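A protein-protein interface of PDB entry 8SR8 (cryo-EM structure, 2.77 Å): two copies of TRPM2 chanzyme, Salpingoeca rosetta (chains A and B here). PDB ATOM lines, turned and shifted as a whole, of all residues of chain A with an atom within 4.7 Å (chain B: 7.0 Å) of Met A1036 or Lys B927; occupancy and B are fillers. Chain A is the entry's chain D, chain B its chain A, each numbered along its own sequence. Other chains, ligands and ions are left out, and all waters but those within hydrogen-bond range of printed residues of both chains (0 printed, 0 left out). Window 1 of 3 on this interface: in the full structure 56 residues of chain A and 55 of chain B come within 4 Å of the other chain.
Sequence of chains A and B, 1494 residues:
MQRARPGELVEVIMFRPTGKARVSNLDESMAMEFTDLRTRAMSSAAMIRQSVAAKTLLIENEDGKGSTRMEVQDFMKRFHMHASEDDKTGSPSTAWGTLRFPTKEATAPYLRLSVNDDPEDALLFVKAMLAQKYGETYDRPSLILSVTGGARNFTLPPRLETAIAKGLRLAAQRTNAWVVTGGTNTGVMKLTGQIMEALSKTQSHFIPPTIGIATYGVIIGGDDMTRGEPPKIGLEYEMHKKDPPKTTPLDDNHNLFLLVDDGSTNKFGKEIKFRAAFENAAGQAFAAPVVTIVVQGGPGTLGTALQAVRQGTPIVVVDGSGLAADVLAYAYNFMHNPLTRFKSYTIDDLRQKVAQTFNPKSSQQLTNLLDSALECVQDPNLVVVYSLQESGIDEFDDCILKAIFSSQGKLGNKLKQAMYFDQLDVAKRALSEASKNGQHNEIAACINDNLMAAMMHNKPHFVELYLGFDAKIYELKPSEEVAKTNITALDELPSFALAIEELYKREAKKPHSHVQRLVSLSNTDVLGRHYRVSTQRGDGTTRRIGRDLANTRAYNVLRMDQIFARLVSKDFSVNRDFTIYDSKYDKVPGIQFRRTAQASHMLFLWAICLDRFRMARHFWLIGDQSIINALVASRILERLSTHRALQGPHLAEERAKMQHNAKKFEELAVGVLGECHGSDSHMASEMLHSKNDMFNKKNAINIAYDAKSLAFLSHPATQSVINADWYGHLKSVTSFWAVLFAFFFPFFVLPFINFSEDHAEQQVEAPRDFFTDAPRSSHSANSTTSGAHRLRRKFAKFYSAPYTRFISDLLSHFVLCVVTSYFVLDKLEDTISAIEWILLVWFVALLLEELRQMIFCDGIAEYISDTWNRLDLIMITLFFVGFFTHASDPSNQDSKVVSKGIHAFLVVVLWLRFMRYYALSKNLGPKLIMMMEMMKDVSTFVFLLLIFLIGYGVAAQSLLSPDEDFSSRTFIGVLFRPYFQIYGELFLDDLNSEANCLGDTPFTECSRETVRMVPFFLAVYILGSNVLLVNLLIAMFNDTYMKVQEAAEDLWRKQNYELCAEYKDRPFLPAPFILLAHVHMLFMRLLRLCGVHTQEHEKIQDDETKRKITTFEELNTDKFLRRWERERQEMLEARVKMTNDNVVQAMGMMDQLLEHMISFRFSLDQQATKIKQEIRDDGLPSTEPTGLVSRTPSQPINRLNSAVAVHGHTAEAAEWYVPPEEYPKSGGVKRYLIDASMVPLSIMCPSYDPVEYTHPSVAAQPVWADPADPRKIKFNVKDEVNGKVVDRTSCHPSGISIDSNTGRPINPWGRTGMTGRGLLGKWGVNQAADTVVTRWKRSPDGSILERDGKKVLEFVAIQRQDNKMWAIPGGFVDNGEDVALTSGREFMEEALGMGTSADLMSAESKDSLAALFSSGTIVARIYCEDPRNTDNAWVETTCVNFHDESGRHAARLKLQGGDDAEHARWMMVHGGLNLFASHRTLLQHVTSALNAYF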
ATOM      1  N   ASP A 937      -1.801 -10.911 -13.908  1.00  0.00           N
ATOM      2  CA  ASP A 937      -2.252  -9.618 -13.384  1.00  0.00           C
ATOM      3  C   ASP A 937      -1.780  -9.385 -11.955  1.00  0.00           C
ATOM      4  O   ASP A 937      -1.527  -8.229 -11.568  1.00  0.00           O
ATOM      5  CB  ASP A 937      -3.763  -9.511 -13.460  1.00  0.00           C
ATOM      6  CG  ASP A 937      -4.251  -9.381 -14.865  1.00  0.00           C
ATOM      7  OD1 ASP A 937      -3.455  -9.020 -15.756  1.00  0.00           O
ATOM      8  OD2 ASP A 937      -5.439  -9.627 -15.082  1.00  0.00           O
ATOM      9  N   THR A 940       1.823  -8.439 -12.274  1.00  0.00           N
ATOM     10  CA  THR A 940       1.846  -7.040 -12.727  1.00  0.00           C
ATOM     11  C   THR A 940       1.660  -6.061 -11.566  1.00  0.00           C
ATOM     12  O   THR A 940       2.401  -5.062 -11.470  1.00  0.00           O
ATOM     13  CB  THR A 940       0.733  -6.856 -13.771  1.00  0.00           C
ATOM     14  OG1 THR A 940       0.989  -7.708 -14.888  1.00  0.00           O
ATOM     15  CG2 THR A 940       0.582  -5.424 -14.276  1.00  0.00           C
ATOM     16  N   LEU A1032      -6.959  -0.577  -9.812  1.00  0.00           N
ATOM     17  CA  LEU A1032      -6.531  -0.963 -11.177  1.00  0.00           C
ATOM     18  C   LEU A1032      -6.470  -2.479 -11.234  1.00  0.00           C
ATOM     19  O   LEU A1032      -6.813  -3.027 -12.269  1.00  0.00           O
ATOM     20  CB  LEU A1032      -5.175  -0.337 -11.483  1.00  0.00           C
ATOM     21  CG  LEU A1032      -4.655  -0.465 -12.911  1.00  0.00           C
ATOM     22  CD1 LEU A1032      -3.839   0.752 -13.299  1.00  0.00           C
ATOM     23  CD2 LEU A1032      -3.812  -1.719 -13.058  1.00  0.00           C
ATOM     24  N   LEU A1033      -6.065  -3.127 -10.159  1.00  0.00           N
ATOM     25  CA  LEU A1033      -6.101  -4.593 -10.099  1.00  0.00           C
ATOM     26  C   LEU A1033      -7.522  -5.135 -10.256  1.00  0.00           C
ATOM     27  O   LEU A1033      -7.707  -6.196 -10.876  1.00  0.00           O
ATOM     28  CB  LEU A1033      -5.440  -5.084  -8.818  1.00  0.00           C
ATOM     29  CG  LEU A1033      -5.253  -6.577  -8.598  1.00  0.00           C
ATOM     30  CD1 LEU A1033      -4.484  -7.175  -9.741  1.00  0.00           C
ATOM     31  CD2 LEU A1033      -4.526  -6.748  -7.358  1.00  0.00           C
ATOM     32  N   ILE A1034      -8.510  -4.430  -9.660  1.00  0.00           N
ATOM     33  CA  ILE A1034      -9.943  -4.756  -9.785  1.00  0.00           C
ATOM     34  C   ILE A1034     -10.395  -4.645 -11.242  1.00  0.00           C
ATOM     35  O   ILE A1034     -11.051  -5.566 -11.766  1.00  0.00           O
ATOM     36  CB  ILE A1034     -10.785  -3.854  -8.852  1.00  0.00           C
ATOM     37  CG1 ILE A1034     -10.529  -4.185  -7.394  1.00  0.00           C
ATOM     38  CG2 ILE A1034     -12.280  -3.948  -9.100  1.00  0.00           C
ATOM     39  CD1 ILE A1034     -11.098  -3.203  -6.406  1.00  0.00           C
ATOM     40  N   ALA A1035      -9.964  -3.557 -11.922  1.00  0.00           N
ATOM     41  CA  ALA A1035     -10.246  -3.315 -13.347  1.00  0.00           C
ATOM     42  C   ALA A1035      -9.612  -4.366 -14.271  1.00  0.00           C
ATOM     43  O   ALA A1035     -10.272  -4.835 -15.222  1.00  0.00           O
ATOM     44  CB  ALA A1035      -9.761  -1.925 -13.730  1.00  0.00           C
ATOM     45  N   MET A1036      -8.341  -4.740 -13.992  1.00  0.00           N
ATOM     46  CA  MET A1036      -7.636  -5.795 -14.735  1.00  0.00           C
ATOM     47  C   MET A1036      -8.271  -7.166 -14.558  1.00  0.00           C
ATOM     48  O   MET A1036      -8.301  -7.947 -15.519  1.00  0.00           O
ATOM     49  CB  MET A1036      -6.158  -5.897 -14.356  1.00  0.00           C
ATOM     50  CG  MET A1036      -5.277  -4.747 -14.740  1.00  0.00           C
ATOM     51  SD  MET A1036      -3.528  -5.086 -14.509  1.00  0.00           S
ATOM     52  CE  MET A1036      -3.364  -5.035 -12.745  1.00  0.00           C
ATOM     53  N   PHE A1037      -8.749  -7.440 -13.341  1.00  0.00           N
ATOM     54  CA  PHE A1037      -9.403  -8.741 -13.053  1.00  0.00           C
ATOM     55  C   PHE A1037     -10.699  -8.815 -13.860  1.00  0.00           C
ATOM     56  O   PHE A1037     -10.894  -9.823 -14.542  1.00  0.00           O
ATOM     57  CB  PHE A1037      -9.678  -8.885 -11.555  1.00  0.00           C
ATOM     58  CG  PHE A1037      -8.582  -9.561 -10.770  1.00  0.00           C
ATOM     59  CD1 PHE A1037      -7.306  -9.693 -11.295  1.00  0.00           C
ATOM     60  CD2 PHE A1037      -8.828 -10.072  -9.507  1.00  0.00           C
ATOM     61  CE1 PHE A1037      -6.302 -10.319 -10.570  1.00  0.00           C
ATOM     62  CE2 PHE A1037      -7.824 -10.696  -8.783  1.00  0.00           C
ATOM     63  CZ  PHE A1037      -6.563 -10.817  -9.316  1.00  0.00           C
ATOM     64  N   ASN A1038     -11.530  -7.771 -13.799  1.00  0.00           N
ATOM     65  CA  ASN A1038     -12.823  -7.774 -14.497  1.00  0.00           C
ATOM     66  C   ASN A1038     -12.665  -7.975 -15.996  1.00  0.00           C
ATOM     67  O   ASN A1038     -13.399  -8.791 -16.576  1.00  0.00           O
ATOM     68  CB  ASN A1038     -13.597  -6.482 -14.253  1.00  0.00           C
ATOM     69  CG  ASN A1038     -14.324  -6.474 -12.945  1.00  0.00           C
ATOM     70  OD1 ASN A1038     -13.995  -5.733 -12.029  1.00  0.00           O
ATOM     71  ND2 ASN A1038     -15.362  -7.278 -12.865  1.00  0.00           N
ATOM     72  N   ASP A1039     -11.669  -7.294 -16.595  1.00  0.00           N
ATOM     73  CA  ASP A1039     -11.359  -7.428 -18.023  1.00  0.00           C
ATOM     74  C   ASP A1039     -10.849  -8.819 -18.392  1.00  0.00           C
ATOM     75  O   ASP A1039     -11.308  -9.409 -19.386  1.00  0.00           O
ATOM     76  CB  ASP A1039     -10.346  -6.386 -18.423  1.00  0.00           C
ATOM     77  CG  ASP A1039      -9.999  -6.460 -19.873  1.00  0.00           C
ATOM     78  OD1 ASP A1039     -10.924  -6.342 -20.699  1.00  0.00           O
ATOM     79  OD2 ASP A1039      -8.808  -6.635 -20.191  1.00  0.00           O
ATOM     80  N   THR A1040      -9.907  -9.341 -17.579  1.00  0.00           N
ATOM     81  CA  THR A1040      -9.288 -10.655 -17.748  1.00  0.00           C
ATOM     82  C   THR A1040     -10.304 -11.781 -17.607  1.00  0.00           C
ATOM     83  O   THR A1040     -10.307 -12.692 -18.448  1.00  0.00           O
ATOM     84  CB  THR A1040      -8.160 -10.789 -16.730  1.00  0.00           C
ATOM     85  OG1 THR A1040      -7.182  -9.786 -17.009  1.00  0.00           O
ATOM     86  CG2 THR A1040      -7.438 -12.118 -16.807  1.00  0.00           C
ATOM     87  N   SER B 921       8.386  -4.290 -21.709  1.00  0.00           N
ATOM     88  CA  SER B 921       7.603  -5.505 -21.530  1.00  0.00           C
ATOM     89  C   SER B 921       6.205  -5.381 -22.114  1.00  0.00           C
ATOM     90  O   SER B 921       5.553  -4.345 -21.993  1.00  0.00           O
ATOM     91  CB  SER B 921       7.500  -5.844 -20.050  1.00  0.00           C
ATOM     92  OG  SER B 921       6.592  -6.907 -19.850  1.00  0.00           O
ATOM     93  N   LYS B 922       5.749  -6.459 -22.766  1.00  0.00           N
ATOM     94  CA  LYS B 922       4.415  -6.532 -23.356  1.00  0.00           C
ATOM     95  C   LYS B 922       3.284  -6.618 -22.337  1.00  0.00           C
ATOM     96  O   LYS B 922       2.131  -6.398 -22.715  1.00  0.00           O
ATOM     97  CB  LYS B 922       4.341  -7.697 -24.345  1.00  0.00           C
ATOM     98  CG  LYS B 922       4.014  -9.050 -23.754  1.00  0.00           C
ATOM     99  CD  LYS B 922       3.625 -10.035 -24.839  1.00  0.00           C
ATOM    100  CE  LYS B 922       4.847 -10.643 -25.493  1.00  0.00           C
ATOM    101  NZ  LYS B 922       5.598 -11.515 -24.549  1.00  0.00           N
ATOM    102  N   ASN B 923       3.568  -6.919 -21.073  1.00  0.00           N
ATOM    103  CA  ASN B 923       2.550  -6.930 -20.049  1.00  0.00           C
ATOM    104  C   ASN B 923       2.551  -5.621 -19.271  1.00  0.00           C
ATOM    105  O   ASN B 923       1.502  -5.012 -19.127  1.00  0.00           O
ATOM    106  CB  ASN B 923       2.798  -8.129 -19.133  1.00  0.00           C
ATOM    107  CG  ASN B 923       1.723  -8.311 -18.110  1.00  0.00           C
ATOM    108  OD1 ASN B 923       0.537  -8.239 -18.419  1.00  0.00           O
ATOM    109  ND2 ASN B 923       2.126  -8.587 -16.882  1.00  0.00           N
ATOM    110  N   LEU B 924       3.718  -5.141 -18.825  1.00  0.00           N
ATOM    111  CA  LEU B 924       3.789  -3.975 -17.941  1.00  0.00           C
ATOM    112  C   LEU B 924       3.631  -2.640 -18.670  1.00  0.00           C
ATOM    113  O   LEU B 924       3.034  -1.699 -18.121  1.00  0.00           O
ATOM    114  CB  LEU B 924       5.118  -3.998 -17.196  1.00  0.00           C
ATOM    115  CG  LEU B 924       5.325  -5.148 -16.218  1.00  0.00           C
ATOM    116  CD1 LEU B 924       6.684  -5.056 -15.595  1.00  0.00           C
ATOM    117  CD2 LEU B 924       4.293  -5.079 -15.133  1.00  0.00           C
ATOM    118  N   GLY B 925       4.094  -2.570 -19.917  1.00  0.00           N
ATOM    119  CA  GLY B 925       4.074  -1.372 -20.752  1.00  0.00           C
ATOM    120  C   GLY B 925       2.736  -0.754 -21.160  1.00  0.00           C
ATOM    121  O   GLY B 925       2.566   0.477 -20.974  1.00  0.00           O
ATOM    122  N   PRO B 926       1.793  -1.544 -21.724  1.00  0.00           N
ATOM    123  CA  PRO B 926       0.484  -1.019 -22.033  1.00  0.00           C
ATOM    124  C   PRO B 926      -0.245  -0.623 -20.748  1.00  0.00           C
ATOM    125  O   PRO B 926      -0.932   0.345 -20.776  1.00  0.00           O
ATOM    126  CB  PRO B 926      -0.196  -2.221 -22.667  1.00  0.00           C
ATOM    127  CG  PRO B 926       0.907  -3.001 -23.282  1.00  0.00           C
ATOM    128  CD  PRO B 926       1.927  -2.945 -22.181  1.00  0.00           C
ATOM    129  N   LYS B 927      -0.087  -1.376 -19.668  1.00  0.00           N
ATOM    130  CA  LYS B 927      -0.704  -1.096 -18.374  1.00  0.00           C
ATOM    131  C   LYS B 927      -0.236   0.246 -17.824  1.00  0.00           C
ATOM    132  O   LYS B 927      -1.018   0.942 -17.167  1.00  0.00           O
ATOM    133  CB  LYS B 927      -0.334  -2.165 -17.358  1.00  0.00           C
ATOM    134  CG  LYS B 927      -1.004  -3.481 -17.530  1.00  0.00           C
ATOM    135  CD  LYS B 927      -2.457  -3.504 -17.721  1.00  0.00           C
ATOM    136  CE  LYS B 927      -2.740  -4.747 -18.554  1.00  0.00           C
ATOM    137  NZ  LYS B 927      -2.061  -5.972 -18.043  1.00  0.00           N
ATOM    138  N   LEU B 928       1.045   0.596 -18.071  1.00  0.00           N
ATOM    139  CA  LEU B 928       1.604   1.907 -17.710  1.00  0.00           C
ATOM    140  C   LEU B 928       0.927   3.043 -18.480  1.00  0.00           C
ATOM    141  O   LEU B 928       0.678   4.127 -17.909  1.00  0.00           O
ATOM    142  CB  LEU B 928       3.108   1.920 -17.954  1.00  0.00           C
ATOM    143  CG  LEU B 928       3.981   1.340 -16.845  1.00  0.00           C
ATOM    144  CD1 LEU B 928       5.434   1.445 -17.225  1.00  0.00           C
ATOM    145  CD2 LEU B 928       3.731   2.021 -15.525  1.00  0.00           C
ATOM    146  N   ILE B 929       0.671   2.810 -19.784  1.00  0.00           N
ATOM    147  CA  ILE B 929      -0.063   3.762 -20.640  1.00  0.00           C
ATOM    148  C   ILE B 929      -1.513   3.943 -20.145  1.00  0.00           C
ATOM    149  O   ILE B 929      -2.037   5.081 -20.114  1.00  0.00           O
ATOM    150  CB  ILE B 929       0.054   3.341 -22.120  1.00  0.00           C
ATOM    151  CG1 ILE B 929       1.506   3.475 -22.550  1.00  0.00           C
ATOM    152  CG2 ILE B 929      -0.764   4.163 -23.075  1.00  0.00           C
ATOM    153  CD1 ILE B 929       1.904   2.545 -23.581  1.00  0.00           C
ATOM    154  N   MET B 930      -2.163   2.821 -19.749  1.00  0.00           N
ATOM    155  CA  MET B 930      -3.509   2.824 -19.144  1.00  0.00           C
ATOM    156  C   MET B 930      -3.553   3.588 -17.825  1.00  0.00           C
ATOM    157  O   MET B 930      -4.543   4.272 -17.579  1.00  0.00           O
ATOM    158  CB  MET B 930      -4.055   1.414 -18.937  1.00  0.00           C
ATOM    159  CG  MET B 930      -4.329   0.690 -20.205  1.00  0.00           C
ATOM    160  SD  MET B 930      -4.550  -1.065 -19.994  1.00  0.00           S
ATOM    161  CE  MET B 930      -4.171  -1.620 -21.643  1.00  0.00           C
ATOM    162  N   MET B 931      -2.483   3.489 -16.996  1.00  0.00           N
ATOM    163  CA  MET B 931      -2.358   4.221 -15.720  1.00  0.00           C
ATOM    164  C   MET B 931      -2.315   5.729 -15.939  1.00  0.00           C
ATOM    165  O   MET B 931      -2.960   6.494 -15.189  1.00  0.00           O
ATOM    166  CB  MET B 931      -1.107   3.793 -14.955  1.00  0.00           C
ATOM    167  CG  MET B 931      -1.204   2.501 -14.200  1.00  0.00           C
ATOM    168  SD  MET B 931       0.372   2.085 -13.438  1.00  0.00           S
ATOM    169  CE  MET B 931       0.685   3.547 -12.464  1.00  0.00           C
ATOM    170  N   MET B 932      -1.540   6.160 -16.959  1.00  0.00           N
ATOM    171  CA  MET B 932      -1.509   7.566 -17.378  1.00  0.00           C
ATOM    172  C   MET B 932      -2.864   8.055 -17.910  1.00  0.00           C
ATOM    173  O   MET B 932      -3.169   9.246 -17.797  1.00  0.00           O
ATOM    174  CB  MET B 932      -0.427   7.786 -18.430  1.00  0.00           C
ATOM    175  CG  MET B 932       0.994   7.563 -17.940  1.00  0.00           C
ATOM    176  SD  MET B 932       1.531   8.704 -16.647  1.00  0.00           S
ATOM    177  CE  MET B 932       1.662   7.610 -15.229  1.00  0.00           C
ATOM    178  N   GLU B 933      -3.656   7.169 -18.537  1.00  0.00           N
ATOM    179  CA  GLU B 933      -5.019   7.542 -18.935  1.00  0.00           C
ATOM    180  C   GLU B 933      -5.963   7.701 -17.733  1.00  0.00           C
ATOM    181  O   GLU B 933      -6.752   8.648 -17.685  1.00  0.00           O
ATOM    182  CB  GLU B 933      -5.579   6.520 -19.911  1.00  0.00           C
ATOM    183  CG  GLU B 933      -5.206   6.777 -21.355  1.00  0.00           C
ATOM    184  CD  GLU B 933      -5.818   8.048 -21.914  1.00  0.00           C
ATOM    185  OE1 GLU B 933      -6.986   8.355 -21.590  1.00  0.00           O
ATOM    186  OE2 GLU B 933      -5.126   8.743 -22.685  1.00  0.00           O
ATOM    187  N   MET B 934      -5.913   6.767 -16.768  1.00  0.00           N
ATOM    188  CA  MET B 934      -6.735   6.781 -15.536  1.00  0.00           C
ATOM    189  C   MET B 934      -6.413   7.899 -14.535  1.00  0.00           C
ATOM    190  O   MET B 934      -7.163   8.025 -13.546  1.00  0.00           O
ATOM    191  CB  MET B 934      -6.864   5.408 -14.878  1.00  0.00           C
ATOM    192  CG  MET B 934      -7.375   4.373 -15.867  1.00  0.00           C
ATOM    193  SD  MET B 934      -8.294   2.949 -15.321  1.00  0.00           S
ATOM    194  CE  MET B 934      -7.021   2.115 -14.436  1.00  0.00           C
ATOM    195  N   ASN B1038     -13.208   0.946 -14.335  1.00  0.00           N
ATOM    196  CA  ASN B1038     -13.669  -0.151 -15.196  1.00  0.00           C
ATOM    197  C   ASN B1038     -14.138   0.344 -16.555  1.00  0.00           C
ATOM    198  O   ASN B1038     -13.758  -0.249 -17.578  1.00  0.00           O
ATOM    199  CB  ASN B1038     -14.800  -0.941 -14.543  1.00  0.00           C
ATOM    200  CG  ASN B1038     -14.312  -1.949 -13.550  1.00  0.00           C
ATOM    201  OD1 ASN B1038     -14.524  -1.828 -12.352  1.00  0.00           O
ATOM    202  ND2 ASN B1038     -13.686  -2.990 -14.056  1.00  0.00           N
ATOM    203  N   TYR B1041     -10.969   1.842 -18.487  1.00  0.00           N
ATOM    204  CA  TYR B1041     -10.134   0.689 -18.859  1.00  0.00           C
ATOM    205  C   TYR B1041     -10.647   0.027 -20.137  1.00  0.00           C
ATOM    206  O   TYR B1041      -9.849  -0.228 -21.062  1.00  0.00           O
ATOM    207  CB  TYR B1041     -10.077  -0.288 -17.686  1.00  0.00           C
ATOM    208  CG  TYR B1041      -8.981  -1.320 -17.764  1.00  0.00           C
ATOM    209  CD1 TYR B1041      -9.171  -2.567 -18.397  1.00  0.00           C
ATOM    210  CD2 TYR B1041      -7.734  -1.035 -17.176  1.00  0.00           C
ATOM    211  CE1 TYR B1041      -8.147  -3.480 -18.466  1.00  0.00           C
ATOM    212  CE2 TYR B1041      -6.702  -1.968 -17.222  1.00  0.00           C
ATOM    213  CZ  TYR B1041      -6.942  -3.178 -17.876  1.00  0.00           C
ATOM    214  OH  TYR B1041      -5.985  -4.129 -17.980  1.00  0.00           O
ATOM    215  N   GLN B1045      -8.185   0.528 -23.612  1.00  0.00           N
ATOM    216  CA  GLN B1045      -7.278  -0.634 -23.682  1.00  0.00           C
ATOM    217  C   GLN B1045      -6.652  -0.903 -25.068  1.00  0.00           C
ATOM    218  O   GLN B1045      -5.433  -1.137 -25.159  1.00  0.00           O
ATOM    219  CB  GLN B1045      -8.069  -1.861 -23.239  1.00  0.00           C
ATOM    220  CG  GLN B1045      -7.301  -3.140 -23.142  1.00  0.00           C
ATOM    221  CD  GLN B1045      -8.166  -4.282 -22.687  1.00  0.00           C
ATOM    222  OE1 GLN B1045      -9.324  -4.089 -22.323  1.00  0.00           O
ATOM    223  NE2 GLN B1045      -7.611  -5.484 -22.695  1.00  0.00           N
ATOM    224  N   ALA B1048      -4.267   2.020 -26.014  1.00  0.00           N
ATOM    225  CA  ALA B1048      -3.053   1.855 -25.217  1.00  0.00           C
ATOM    226  C   ALA B1048      -2.117   0.803 -25.792  1.00  0.00           C
ATOM    227  O   ALA B1048      -0.891   0.980 -25.746  1.00  0.00           O
ATOM    228  CB  ALA B1048      -3.425   1.495 -23.790  1.00  0.00           C
ATOM    229  N   GLU B1049      -2.691  -0.311 -26.288  1.00  0.00           N
ATOM    230  CA  GLU B1049      -1.926  -1.372 -26.953  1.00  0.00           C
ATOM    231  C   GLU B1049      -1.251  -0.890 -28.244  1.00  0.00           C
ATOM    232  O   GLU B1049      -0.079  -1.223 -28.498  1.00  0.00           O
ATOM    233  CB  GLU B1049      -2.845  -2.553 -27.235  1.00  0.00           C
ATOM    234  CG  GLU B1049      -2.126  -3.841 -27.499  1.00  0.00           C
ATOM    235  CD  GLU B1049      -1.539  -4.464 -26.249  1.00  0.00           C
ATOM    236  OE1 GLU B1049      -2.099  -4.256 -25.152  1.00  0.00           O
ATOM    237  OE2 GLU B1049      -0.514  -5.166 -26.366  1.00  0.00           O
ATOM    238  N   TRP B1052       1.549   1.547 -27.358  1.00  0.00           N
ATOM    239  CA  TRP B1052       2.698   0.764 -26.888  1.00  0.00           C
ATOM    240  C   TRP B1052       3.487   0.193 -28.067  1.00  0.00           C
ATOM    241  O   TRP B1052       4.725   0.154 -28.022  1.00  0.00           O
ATOM    242  CB  TRP B1052       2.265  -0.384 -25.951  1.00  0.00           C
ATOM    243  CG  TRP B1052       3.451  -1.211 -25.489  1.00  0.00           C
ATOM    244  CD1 TRP B1052       4.386  -0.834 -24.581  1.00  0.00           C
ATOM    245  CD2 TRP B1052       3.898  -2.466 -26.019  1.00  0.00           C
ATOM    246  NE1 TRP B1052       5.358  -1.787 -24.470  1.00  0.00           N
ATOM    247  CE2 TRP B1052       5.092  -2.795 -25.353  1.00  0.00           C
ATOM    248  CE3 TRP B1052       3.410  -3.331 -27.010  1.00  0.00           C
ATOM    249  CZ2 TRP B1052       5.794  -3.966 -25.619  1.00  0.00           C
ATOM    250  CZ3 TRP B1052       4.102  -4.509 -27.269  1.00  0.00           C
ATOM    251  CH2 TRP B1052       5.282  -4.815 -26.569  1.00  0.00           C
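Of the 11 printed residues of chain A, 6 touch a printed residue of chain B. Among the printed residues, no Asp or Glu carboxylate lies within 4 Å of a Lys or Arg side-chain nitrogen of the other chain.
Asn B1038 touches its own counterpart, Asn A1038. Position printed for both chains: 1038.
The side-chain hydroxyl (OG) of Ser B921 lies close to the backbone NH (N) of Asn B923, at 3.3 Å. The side-chain amide oxygen of Asn B923 sits at hydrogen-bond distance from the side-chain amino group of Lys B927 (3.5 Å). O of Ile A1034 sits close to OD1 of Asn A1038, at 3.0 Å. O of Met A1036 lies within hydrogen-bond range of OG1 of Thr A1040 (2.6 Å).
Among the printed residues, pairs that only touch across the chains: Leu A1032 with Met B931 (3.3 Å), Met A1036 with Tyr B1041 (3.4 Å), Ala A1035 with Asn B1038 (3.5 Å), Leu A1032 with Met B934 (3.6 Å), Asp A1039 with Tyr B1041 (3.6 Å), Met A1036 with Lys B927 (3.7 Å) and Thr A940 with Leu B924 (3.8 Å).
Of the printed residues of chain B, Leu A1032 touches Met B931 (3.3 Å) and Met B934 (3.6 Å). Met A1036 touches two residues of chain B. Of the printed residues of chain B, Asp A1039 touches Tyr B1041 and Gln B1045. Printed residues of chain A within 4 Å of Leu B924: Thr A940 (3.8 Å). Leu B928 touches none of the printed residues of chain A. Met B930 touches none of the printed residues of chain A. Of the printed residues of chain A, Met B931 touches Leu A1032 (3.3 Å). Of the printed residues of chain A, Asn B1038 touches Ala A1035 (3.5 Å) and Asn A1038 (3.4 Å). The nearest residue of chain A that does not touch Lys B927 is Asp A937 (4.1 Å). The nearest printed residue of chain A that does not touch Tyr B1041 is Ala A1035 (4.1 Å).
OG1 of Thr A940 sits at hydrogen-bond distance from ND2 of Asn B923 (2.5 Å). ND2 of Asn B1038 sits at hydrogen-bond distance from OD1 of Asn A1038, at 3.4 Å. The side-chain carboxylate (OD2) of Asp A1039 is in hydrogen-bond range of the side-chain amide nitrogen (NE2) of Gln B1045.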
